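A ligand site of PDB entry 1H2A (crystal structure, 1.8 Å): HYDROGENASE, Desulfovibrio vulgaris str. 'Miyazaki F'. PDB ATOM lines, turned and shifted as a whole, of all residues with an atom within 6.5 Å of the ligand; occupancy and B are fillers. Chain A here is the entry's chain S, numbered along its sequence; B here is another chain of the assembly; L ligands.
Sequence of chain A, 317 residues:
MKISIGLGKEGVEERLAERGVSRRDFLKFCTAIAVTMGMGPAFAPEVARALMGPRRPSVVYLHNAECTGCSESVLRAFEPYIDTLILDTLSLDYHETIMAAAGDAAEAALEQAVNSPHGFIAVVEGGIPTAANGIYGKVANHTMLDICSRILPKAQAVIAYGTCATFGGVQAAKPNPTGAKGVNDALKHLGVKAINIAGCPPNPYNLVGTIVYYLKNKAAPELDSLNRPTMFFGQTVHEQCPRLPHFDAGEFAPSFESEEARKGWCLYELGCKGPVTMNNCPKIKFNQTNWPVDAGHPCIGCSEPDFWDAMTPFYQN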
ATOM      1  N   ALA A  65      22.759   9.679 -10.190  1.00  0.00           N
ATOM      2  CA  ALA A  65      24.207   9.460 -10.411  1.00  0.00           C
ATOM      3  C   ALA A  65      24.292   8.251 -11.336  1.00  0.00           C
ATOM      4  O   ALA A  65      24.141   7.117 -10.886  1.00  0.00           O
ATOM      5  CB  ALA A  65      24.927   9.168  -9.076  1.00  0.00           C
ATOM      6  N   GLU A  66      24.558   8.491 -12.608  1.00  0.00           N
ATOM      7  CA  GLU A  66      24.572   7.405 -13.567  1.00  0.00           C
ATOM      8  C   GLU A  66      25.403   7.635 -14.832  1.00  0.00           C
ATOM      9  O   GLU A  66      25.883   8.756 -15.079  1.00  0.00           O
ATOM     10  CB  GLU A  66      23.128   7.059 -13.953  1.00  0.00           C
ATOM     11  CG  GLU A  66      22.218   8.283 -14.197  1.00  0.00           C
ATOM     12  CD  GLU A  66      22.485   8.996 -15.513  1.00  0.00           C
ATOM     13  OE1 GLU A  66      22.520   8.298 -16.548  1.00  0.00           O
ATOM     14  OE2 GLU A  66      22.660  10.238 -15.546  1.00  0.00           O
ATOM     15  N   CYS A  67      25.539   6.569 -15.629  1.00  0.00           N
ATOM     16  CA  CYS A  67      26.291   6.573 -16.893  1.00  0.00           C
ATOM     17  C   CYS A  67      25.363   6.404 -18.105  1.00  0.00           C
ATOM     18  O   CYS A  67      25.845   6.220 -19.226  1.00  0.00           O
ATOM     19  CB  CYS A  67      27.329   5.414 -16.920  1.00  0.00           C
ATOM     20  SG  CYS A  67      26.587   3.726 -17.012  1.00  0.00           S
ATOM     21  N   THR A  68      24.056   6.329 -17.862  1.00  0.00           N
ATOM     22  CA  THR A  68      23.021   6.171 -18.897  1.00  0.00           C
ATOM     23  C   THR A  68      22.945   4.786 -19.554  1.00  0.00           C
ATOM     24  O   THR A  68      22.069   4.527 -20.394  1.00  0.00           O
ATOM     25  CB  THR A  68      23.121   7.264 -19.958  1.00  0.00           C
ATOM     26  OG1 THR A  68      23.340   8.521 -19.288  1.00  0.00           O
ATOM     27  CG2 THR A  68      21.823   7.362 -20.795  1.00  0.00           C
ATOM     28  N   GLY A  69      23.840   3.893 -19.143  1.00  0.00           N
ATOM     29  CA  GLY A  69      23.866   2.554 -19.690  1.00  0.00           C
ATOM     30  C   GLY A  69      22.592   1.797 -19.438  1.00  0.00           C
ATOM     31  O   GLY A  69      22.267   0.845 -20.154  1.00  0.00           O
ATOM     32  N   CYS A  70      21.854   2.188 -18.418  1.00  0.00           N
ATOM     33  CA  CYS A  70      20.588   1.520 -18.122  1.00  0.00           C
ATOM     34  C   CYS A  70      19.505   2.042 -19.118  1.00  0.00           C
ATOM     35  O   CYS A  70      18.724   1.266 -19.660  1.00  0.00           O
ATOM     36  CB  CYS A  70      20.170   1.737 -16.656  1.00  0.00           C
ATOM     37  SG  CYS A  70      21.165   0.837 -15.428  1.00  0.00           S
ATOM     38  N   SER A  71      19.492   3.341 -19.381  1.00  0.00           N
ATOM     39  CA  SER A  71      18.546   3.894 -20.339  1.00  0.00           C
ATOM     40  C   SER A  71      18.793   3.176 -21.685  1.00  0.00           C
ATOM     41  O   SER A  71      17.874   2.630 -22.303  1.00  0.00           O
ATOM     42  CB  SER A  71      18.757   5.397 -20.503  1.00  0.00           C
ATOM     43  OG  SER A  71      18.156   6.114 -19.445  1.00  0.00           O
ATOM     44  N   GLU A 125      17.012   5.934 -12.319  1.00  0.00           N
ATOM     45  CA  GLU A 125      18.304   5.434 -12.792  1.00  0.00           C
ATOM     46  C   GLU A 125      19.476   6.127 -12.073  1.00  0.00           C
ATOM     47  O   GLU A 125      19.657   7.357 -12.211  1.00  0.00           O
ATOM     48  CB  GLU A 125      18.458   5.614 -14.306  1.00  0.00           C
ATOM     49  CG  GLU A 125      19.818   5.181 -14.832  1.00  0.00           C
ATOM     50  CD  GLU A 125      19.951   5.255 -16.353  1.00  0.00           C
ATOM     51  OE1 GLU A 125      18.941   5.509 -17.047  1.00  0.00           O
ATOM     52  OE2 GLU A 125      21.080   5.032 -16.861  1.00  0.00           O
ATOM     53  N   GLY A 126      20.244   5.365 -11.312  1.00  0.00           N
ATOM     54  CA  GLY A 126      21.394   5.940 -10.639  1.00  0.00           C
ATOM     55  C   GLY A 126      21.305   6.072  -9.126  1.00  0.00           C
ATOM     56  O   GLY A 126      20.218   5.990  -8.554  1.00  0.00           O
ATOM     57  N   TYR A 161      16.014   1.202 -11.268  1.00  0.00           N
ATOM     58  CA  TYR A 161      16.502   0.417 -12.376  1.00  0.00           C
ATOM     59  C   TYR A 161      18.008   0.458 -12.449  1.00  0.00           C
ATOM     60  O   TYR A 161      18.596   1.524 -12.643  1.00  0.00           O
ATOM     61  CB  TYR A 161      15.858   0.875 -13.689  1.00  0.00           C
ATOM     62  CG  TYR A 161      16.124  -0.051 -14.876  1.00  0.00           C
ATOM     63  CD1 TYR A 161      15.780  -1.392 -14.819  1.00  0.00           C
ATOM     64  CD2 TYR A 161      16.761   0.409 -16.042  1.00  0.00           C
ATOM     65  CE1 TYR A 161      16.068  -2.272 -15.895  1.00  0.00           C
ATOM     66  CE2 TYR A 161      17.053  -0.445 -17.102  1.00  0.00           C
ATOM     67  CZ  TYR A 161      16.711  -1.791 -17.024  1.00  0.00           C
ATOM     68  OH  TYR A 161      17.041  -2.681 -18.036  1.00  0.00           O
ATOM     69  N   GLY A 162      18.625  -0.694 -12.208  1.00  0.00           N
ATOM     70  CA  GLY A 162      20.072  -0.803 -12.258  1.00  0.00           C
ATOM     71  C   GLY A 162      20.712  -0.926 -10.899  1.00  0.00           C
ATOM     72  O   GLY A 162      20.132  -0.560  -9.878  1.00  0.00           O
ATOM     73  N   THR A 163      21.974  -1.334 -10.894  1.00  0.00           N
ATOM     74  CA  THR A 163      22.715  -1.526  -9.647  1.00  0.00           C
ATOM     75  C   THR A 163      22.983  -0.242  -8.858  1.00  0.00           C
ATOM     76  O   THR A 163      22.973  -0.252  -7.617  1.00  0.00           O
ATOM     77  CB  THR A 163      23.989  -2.321  -9.924  1.00  0.00           C
ATOM     78  OG1 THR A 163      23.676  -3.715  -9.919  1.00  0.00           O
ATOM     79  CG2 THR A 163      25.086  -1.966  -8.900  1.00  0.00           C
ATOM     80  N   CYS A 164      23.206   0.864  -9.557  1.00  0.00           N
ATOM     81  CA  CYS A 164      23.423   2.148  -8.912  1.00  0.00           C
ATOM     82  C   CYS A 164      22.216   2.602  -8.064  1.00  0.00           C
ATOM     83  O   CYS A 164      22.377   2.959  -6.896  1.00  0.00           O
ATOM     84  CB  CYS A 164      23.722   3.220  -9.943  1.00  0.00           C
ATOM     85  SG  CYS A 164      25.265   2.997 -10.887  1.00  0.00           S
ATOM     86  N   ALA A 165      21.027   2.577  -8.666  1.00  0.00           N
ATOM     87  CA  ALA A 165      19.791   3.014  -7.986  1.00  0.00           C
ATOM     88  C   ALA A 165      19.432   2.031  -6.901  1.00  0.00           C
ATOM     89  O   ALA A 165      19.075   2.396  -5.786  1.00  0.00           O
ATOM     90  CB  ALA A 165      18.634   3.123  -8.992  1.00  0.00           C
ATOM     91  N   GLY A 169      25.889   1.273  -6.349  1.00  0.00           N
ATOM     92  CA  GLY A 169      26.762   1.157  -7.500  1.00  0.00           C
ATOM     93  C   GLY A 169      28.178   1.691  -7.499  1.00  0.00           C
ATOM     94  O   GLY A 169      28.764   2.061  -6.457  1.00  0.00           O
ATOM     95  N   VAL A 170      28.714   1.747  -8.721  1.00  0.00           N
ATOM     96  CA  VAL A 170      30.090   2.135  -8.957  1.00  0.00           C
ATOM     97  C   VAL A 170      30.599   3.313  -8.166  1.00  0.00           C
ATOM     98  O   VAL A 170      31.724   3.289  -7.705  1.00  0.00           O
ATOM     99  CB  VAL A 170      30.380   2.342 -10.483  1.00  0.00           C
ATOM    100  CG1 VAL A 170      29.720   3.615 -11.020  1.00  0.00           C
ATOM    101  CG2 VAL A 170      31.881   2.375 -10.733  1.00  0.00           C
ATOM    102  N   GLN A 171      29.779   4.351  -8.000  1.00  0.00           N
ATOM    103  CA  GLN A 171      30.225   5.539  -7.267  1.00  0.00           C
ATOM    104  C   GLN A 171      30.132   5.405  -5.736  1.00  0.00           C
ATOM    105  O   GLN A 171      30.601   6.276  -5.005  1.00  0.00           O
ATOM    106  CB  GLN A 171      29.488   6.795  -7.746  1.00  0.00           C
ATOM    107  CG  GLN A 171      27.953   6.790  -7.565  1.00  0.00           C
ATOM    108  CD  GLN A 171      27.212   6.302  -8.805  1.00  0.00           C
ATOM    109  OE1 GLN A 171      27.389   6.855  -9.887  1.00  0.00           O
ATOM    110  NE2 GLN A 171      26.362   5.272  -8.648  1.00  0.00           N
ATOM    111  N   GLY A 199      21.436  -5.174 -11.849  1.00  0.00           N
ATOM    112  CA  GLY A 199      22.199  -5.537 -13.040  1.00  0.00           C
ATOM    113  C   GLY A 199      22.960  -4.303 -13.473  1.00  0.00           C
ATOM    114  O   GLY A 199      22.555  -3.207 -13.079  1.00  0.00           O
ATOM    115  N   CYS A 200      23.968  -4.423 -14.334  1.00  0.00           N
ATOM    116  CA  CYS A 200      24.744  -3.258 -14.749  1.00  0.00           C
ATOM    117  C   CYS A 200      25.146  -3.249 -16.241  1.00  0.00           C
ATOM    118  O   CYS A 200      26.316  -3.429 -16.588  1.00  0.00           O
ATOM    119  CB  CYS A 200      25.987  -3.137 -13.831  1.00  0.00           C
ATOM    120  SG  CYS A 200      26.850  -1.530 -13.833  1.00  0.00           S
ATOM    121  N   PRO A 201      24.186  -2.976 -17.132  1.00  0.00           N
ATOM    122  CA  PRO A 201      22.775  -2.688 -16.893  1.00  0.00           C
ATOM    123  C   PRO A 201      21.995  -3.981 -16.750  1.00  0.00           C
ATOM    124  O   PRO A 201      22.517  -5.070 -17.031  1.00  0.00           O
ATOM    125  CB  PRO A 201      22.388  -1.919 -18.156  1.00  0.00           C
ATOM    126  CG  PRO A 201      23.200  -2.619 -19.226  1.00  0.00           C
ATOM    127  CD  PRO A 201      24.534  -2.824 -18.571  1.00  0.00           C
ATOM    128  N   PRO A 202      20.765  -3.907 -16.207  1.00  0.00           N
ATOM    129  CA  PRO A 202      19.915  -5.079 -16.034  1.00  0.00           C
ATOM    130  C   PRO A 202      19.479  -5.556 -17.427  1.00  0.00           C
ATOM    131  O   PRO A 202      19.633  -4.822 -18.397  1.00  0.00           O
ATOM    132  CB  PRO A 202      18.694  -4.525 -15.284  1.00  0.00           C
ATOM    133  CG  PRO A 202      19.205  -3.296 -14.619  1.00  0.00           C
ATOM    134  CD  PRO A 202      20.128  -2.703 -15.649  1.00  0.00           C
ATOM    135  N   CYS A 302      27.722  -8.490 -11.291  1.00  0.00           N
ATOM    136  CA  CYS A 302      27.198  -7.136 -11.406  1.00  0.00           C
ATOM    137  C   CYS A 302      25.786  -6.834 -10.863  1.00  0.00           C
ATOM    138  O   CYS A 302      25.383  -5.671 -10.798  1.00  0.00           O
ATOM    139  CB  CYS A 302      27.314  -6.648 -12.860  1.00  0.00           C
ATOM    140  SG  CYS A 302      26.070  -7.309 -14.018  1.00  0.00           S
ATOM    141  N   TRP A 308      31.367  -4.138  -6.224  1.00  0.00           N
ATOM    142  CA  TRP A 308      32.665  -3.518  -6.521  1.00  0.00           C
ATOM    143  C   TRP A 308      33.768  -3.811  -5.488  1.00  0.00           C
ATOM    144  O   TRP A 308      34.935  -4.010  -5.863  1.00  0.00           O
ATOM    145  CB  TRP A 308      32.514  -2.017  -6.729  1.00  0.00           C
ATOM    146  CG  TRP A 308      31.616  -1.679  -7.872  1.00  0.00           C
ATOM    147  CD1 TRP A 308      30.359  -1.135  -7.797  1.00  0.00           C
ATOM    148  CD2 TRP A 308      31.884  -1.857  -9.280  1.00  0.00           C
ATOM    149  NE1 TRP A 308      29.836  -0.976  -9.059  1.00  0.00           N
ATOM    150  CE2 TRP A 308      30.750  -1.393  -9.987  1.00  0.00           C
ATOM    151  CE3 TRP A 308      32.982  -2.349 -10.005  1.00  0.00           C
ATOM    152  CZ2 TRP A 308      30.676  -1.418 -11.388  1.00  0.00           C
ATOM    153  CZ3 TRP A 308      32.907  -2.381 -11.394  1.00  0.00           C
ATOM    154  CH2 TRP A 308      31.759  -1.912 -12.066  1.00  0.00           C
ATOM    155  N   ARG B  59      31.278  12.047  -9.733  1.00  0.00           N
ATOM    156  CA  ARG B  59      31.263  10.688  -9.229  1.00  0.00           C
ATOM    157  C   ARG B  59      32.625  10.286  -8.621  1.00  0.00           C
ATOM    158  O   ARG B  59      32.673   9.472  -7.694  1.00  0.00           O
ATOM    159  CB  ARG B  59      30.843   9.724 -10.338  1.00  0.00           C
ATOM    160  CG  ARG B  59      29.339   9.759 -10.681  1.00  0.00           C
ATOM    161  CD  ARG B  59      28.966   8.734 -11.740  1.00  0.00           C
ATOM    162  NE  ARG B  59      29.654   9.079 -12.984  1.00  0.00           N
ATOM    163  CZ  ARG B  59      29.784   8.279 -14.029  1.00  0.00           C
ATOM    164  NH1 ARG B  59      29.276   7.056 -14.009  1.00  0.00           N
ATOM    165  NH2 ARG B  59      30.471   8.706 -15.086  1.00  0.00           N
ATOM    166  N   ARG B  79      32.051   1.874 -16.746  1.00  0.00           N
ATOM    167  CA  ARG B  79      30.852   2.492 -16.163  1.00  0.00           C
ATOM    168  C   ARG B  79      30.935   4.023 -16.126  1.00  0.00           C
ATOM    169  O   ARG B  79      30.136   4.682 -15.465  1.00  0.00           O
ATOM    170  CB  ARG B  79      30.538   1.949 -14.769  1.00  0.00           C
ATOM    171  CG  ARG B  79      30.800   0.460 -14.543  1.00  0.00           C
ATOM    172  CD  ARG B  79      29.894  -0.552 -15.292  1.00  0.00           C
ATOM    173  NE  ARG B  79      30.726  -1.435 -16.080  1.00  0.00           N
ATOM    174  CZ  ARG B  79      30.521  -2.736 -16.282  1.00  0.00           C
ATOM    175  NH1 ARG B  79      29.479  -3.365 -15.761  1.00  0.00           N
ATOM    176  NH2 ARG B  79      31.418  -3.427 -16.944  1.00  0.00           N
ATOM    177  N   THR B  80      31.941   4.584 -16.772  1.00  0.00           N
ATOM    178  CA  THR B  80      32.039   6.035 -16.863  1.00  0.00           C
ATOM    179  C   THR B  80      30.915   6.445 -17.838  1.00  0.00           C
ATOM    180  O   THR B  80      30.461   7.606 -17.853  1.00  0.00           O
ATOM    181  CB  THR B  80      33.391   6.429 -17.516  1.00  0.00           C
ATOM    182  OG1 THR B  80      34.478   5.891 -16.750  1.00  0.00           O
ATOM    183  CG2 THR B  80      33.543   7.919 -17.660  1.00  0.00           C
ATOM    184  N   CYS B  81      30.491   5.507 -18.686  1.00  0.00           N
ATOM    185  CA  CYS B  81      29.460   5.785 -19.664  1.00  0.00           C
ATOM    186  C   CYS B  81      28.792   4.574 -20.308  1.00  0.00           C
ATOM    187  O   CYS B  81      29.411   3.486 -20.448  1.00  0.00           O
ATOM    188  CB  CYS B  81      30.017   6.684 -20.738  1.00  0.00           C
ATOM    189  SG  CYS B  81      28.639   7.356 -21.708  1.00  0.00           S
ATOM    190  N   GLY B  82      27.514   4.730 -20.675  1.00  0.00           N
ATOM    191  CA  GLY B  82      26.776   3.639 -21.288  1.00  0.00           C
ATOM    192  C   GLY B  82      26.358   3.983 -22.720  1.00  0.00           C
ATOM    193  O   GLY B  82      25.932   3.142 -23.480  1.00  0.00           O
ATOM    194  N   PRO B 234      24.395  -2.663 -23.695  1.00  0.00           N
ATOM    195  CA  PRO B 234      25.578  -1.927 -23.262  1.00  0.00           C
ATOM    196  C   PRO B 234      26.492  -2.746 -22.363  1.00  0.00           C
ATOM    197  O   PRO B 234      26.084  -3.753 -21.756  1.00  0.00           O
ATOM    198  CB  PRO B 234      24.982  -0.765 -22.444  1.00  0.00           C
ATOM    199  CG  PRO B 234      23.499  -0.788 -22.761  1.00  0.00           C
ATOM    200  CD  PRO B 234      23.224  -2.247 -22.914  1.00  0.00           C
ATOM    201  N   HIS B 235      27.736  -2.287 -22.299  1.00  0.00           N
ATOM    202  CA  HIS B 235      28.782  -2.864 -21.462  1.00  0.00           C
ATOM    203  C   HIS B 235      29.232  -4.263 -21.782  1.00  0.00           C
ATOM    204  O   HIS B 235      28.830  -5.276 -21.186  1.00  0.00           O
ATOM    205  CB  HIS B 235      28.434  -2.666 -19.992  1.00  0.00           C
ATOM    206  CG  HIS B 235      28.381  -1.228 -19.603  1.00  0.00           C
ATOM    207  ND1 HIS B 235      27.720  -0.771 -18.480  1.00  0.00           N
ATOM    208  CD2 HIS B 235      28.944  -0.131 -20.176  1.00  0.00           C
ATOM    209  CE1 HIS B 235      27.879   0.544 -18.373  1.00  0.00           C
ATOM    210  NE2 HIS B 235      28.611   0.960 -19.400  1.00  0.00           N
HETATM  211 FE1  LIG L   1      25.525   2.436 -15.605  1.00  0.00          FE
HETATM  212 FE2  LIG L   1      24.767   2.258 -13.071  1.00  0.00          FE
HETATM  213 FE3  LIG L   1      25.732   0.409 -14.410  1.00  0.00          FE
HETATM  214 FE4  LIG L   1      23.363   1.321 -14.915  1.00  0.00          FE
HETATM  215  S1  LIG L   1      23.979   0.245 -12.922  1.00  0.00           S
HETATM  216  S2  LIG L   1      24.866   0.503 -16.554  1.00  0.00           S
HETATM  217  S3  LIG L   1      23.656   3.520 -14.765  1.00  0.00           S
HETATM  218  S4  LIG L   1      26.897   2.168 -13.851  1.00  0.00           S
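The backbone NH of Cys 67 lies close to a sulfur (S3) of the ligand (3.7 Å).
The side-chain sulfur (SG) of Cys 67 is bound to an iron atom (FE1) of the ligand (2.2 Å).
The side-chain sulfur of Cys 70 binds an iron atom (FE4) of the ligand, at 2.3 Å.
The side-chain sulfur (SG) of Cys 200 is bound to an iron atom (FE3) of the ligand, at 2.3 Å.
A sulfur (S1) of the ligand sits close to the backbone NH of Cys 164 (3.5 Å).
SG of Cys 164 binds FE2 of the ligand, at 2.4 Å.
S1 of the ligand lies close to N of Thr 163, at 3.3 Å.
A sulfur (S2) of the ligand lies close to a ring nitrogen (ND1) of His 235 of chain B (3.7 Å).
The side-chain sulfur of Cys 67 sits close to the backbone NH of Gly 69 (3.5 Å).
The backbone carbonyl oxygen (O) of Cys 67 lies within hydrogen-bond range of the backbone NH (N) of Gly 82 of chain B, 2.7 Å away.
The backbone NH of Thr 163 sits at hydrogen-bond distance from the backbone carbonyl oxygen of Gly 199 (2.9 Å).
OG1 of Thr 163 sits at hydrogen-bond distance from O of Cys 302, 2.7 Å away.
NE2 of His 235 of chain B is in hydrogen-bond range of O of Cys 81 of chain B, 2.8 Å away.
The side-chain hydroxyl of Ser 71 is in hydrogen-bond range of the side-chain carboxylate of Glu 125 (2.6 Å).
OE1 of Glu 66 lies within hydrogen-bond range of N of Thr 68, at 2.8 Å.
The backbone carbonyl oxygen of Arg 79 of chain B is in hydrogen-bond range of the guanidinium group of Arg 59 of chain B (2.9 Å).
OE2 of Glu 125 sits close to S3 of the ligand.
O of Gly 199 lies close to S1 of the ligand (3.7 Å).
A sulfur (S2) of the ligand sits close to the backbone nitrogen of Pro 201.
Glu 66 touches the ligand.
Gly 69 touches the ligand.
CB of Arg 79 of chain B touches S4 of the ligand (3.8 Å).
Hydrophobic or aromatic side chains within 4 Å of the ligand: Pro 201 and His 235 of chain B.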
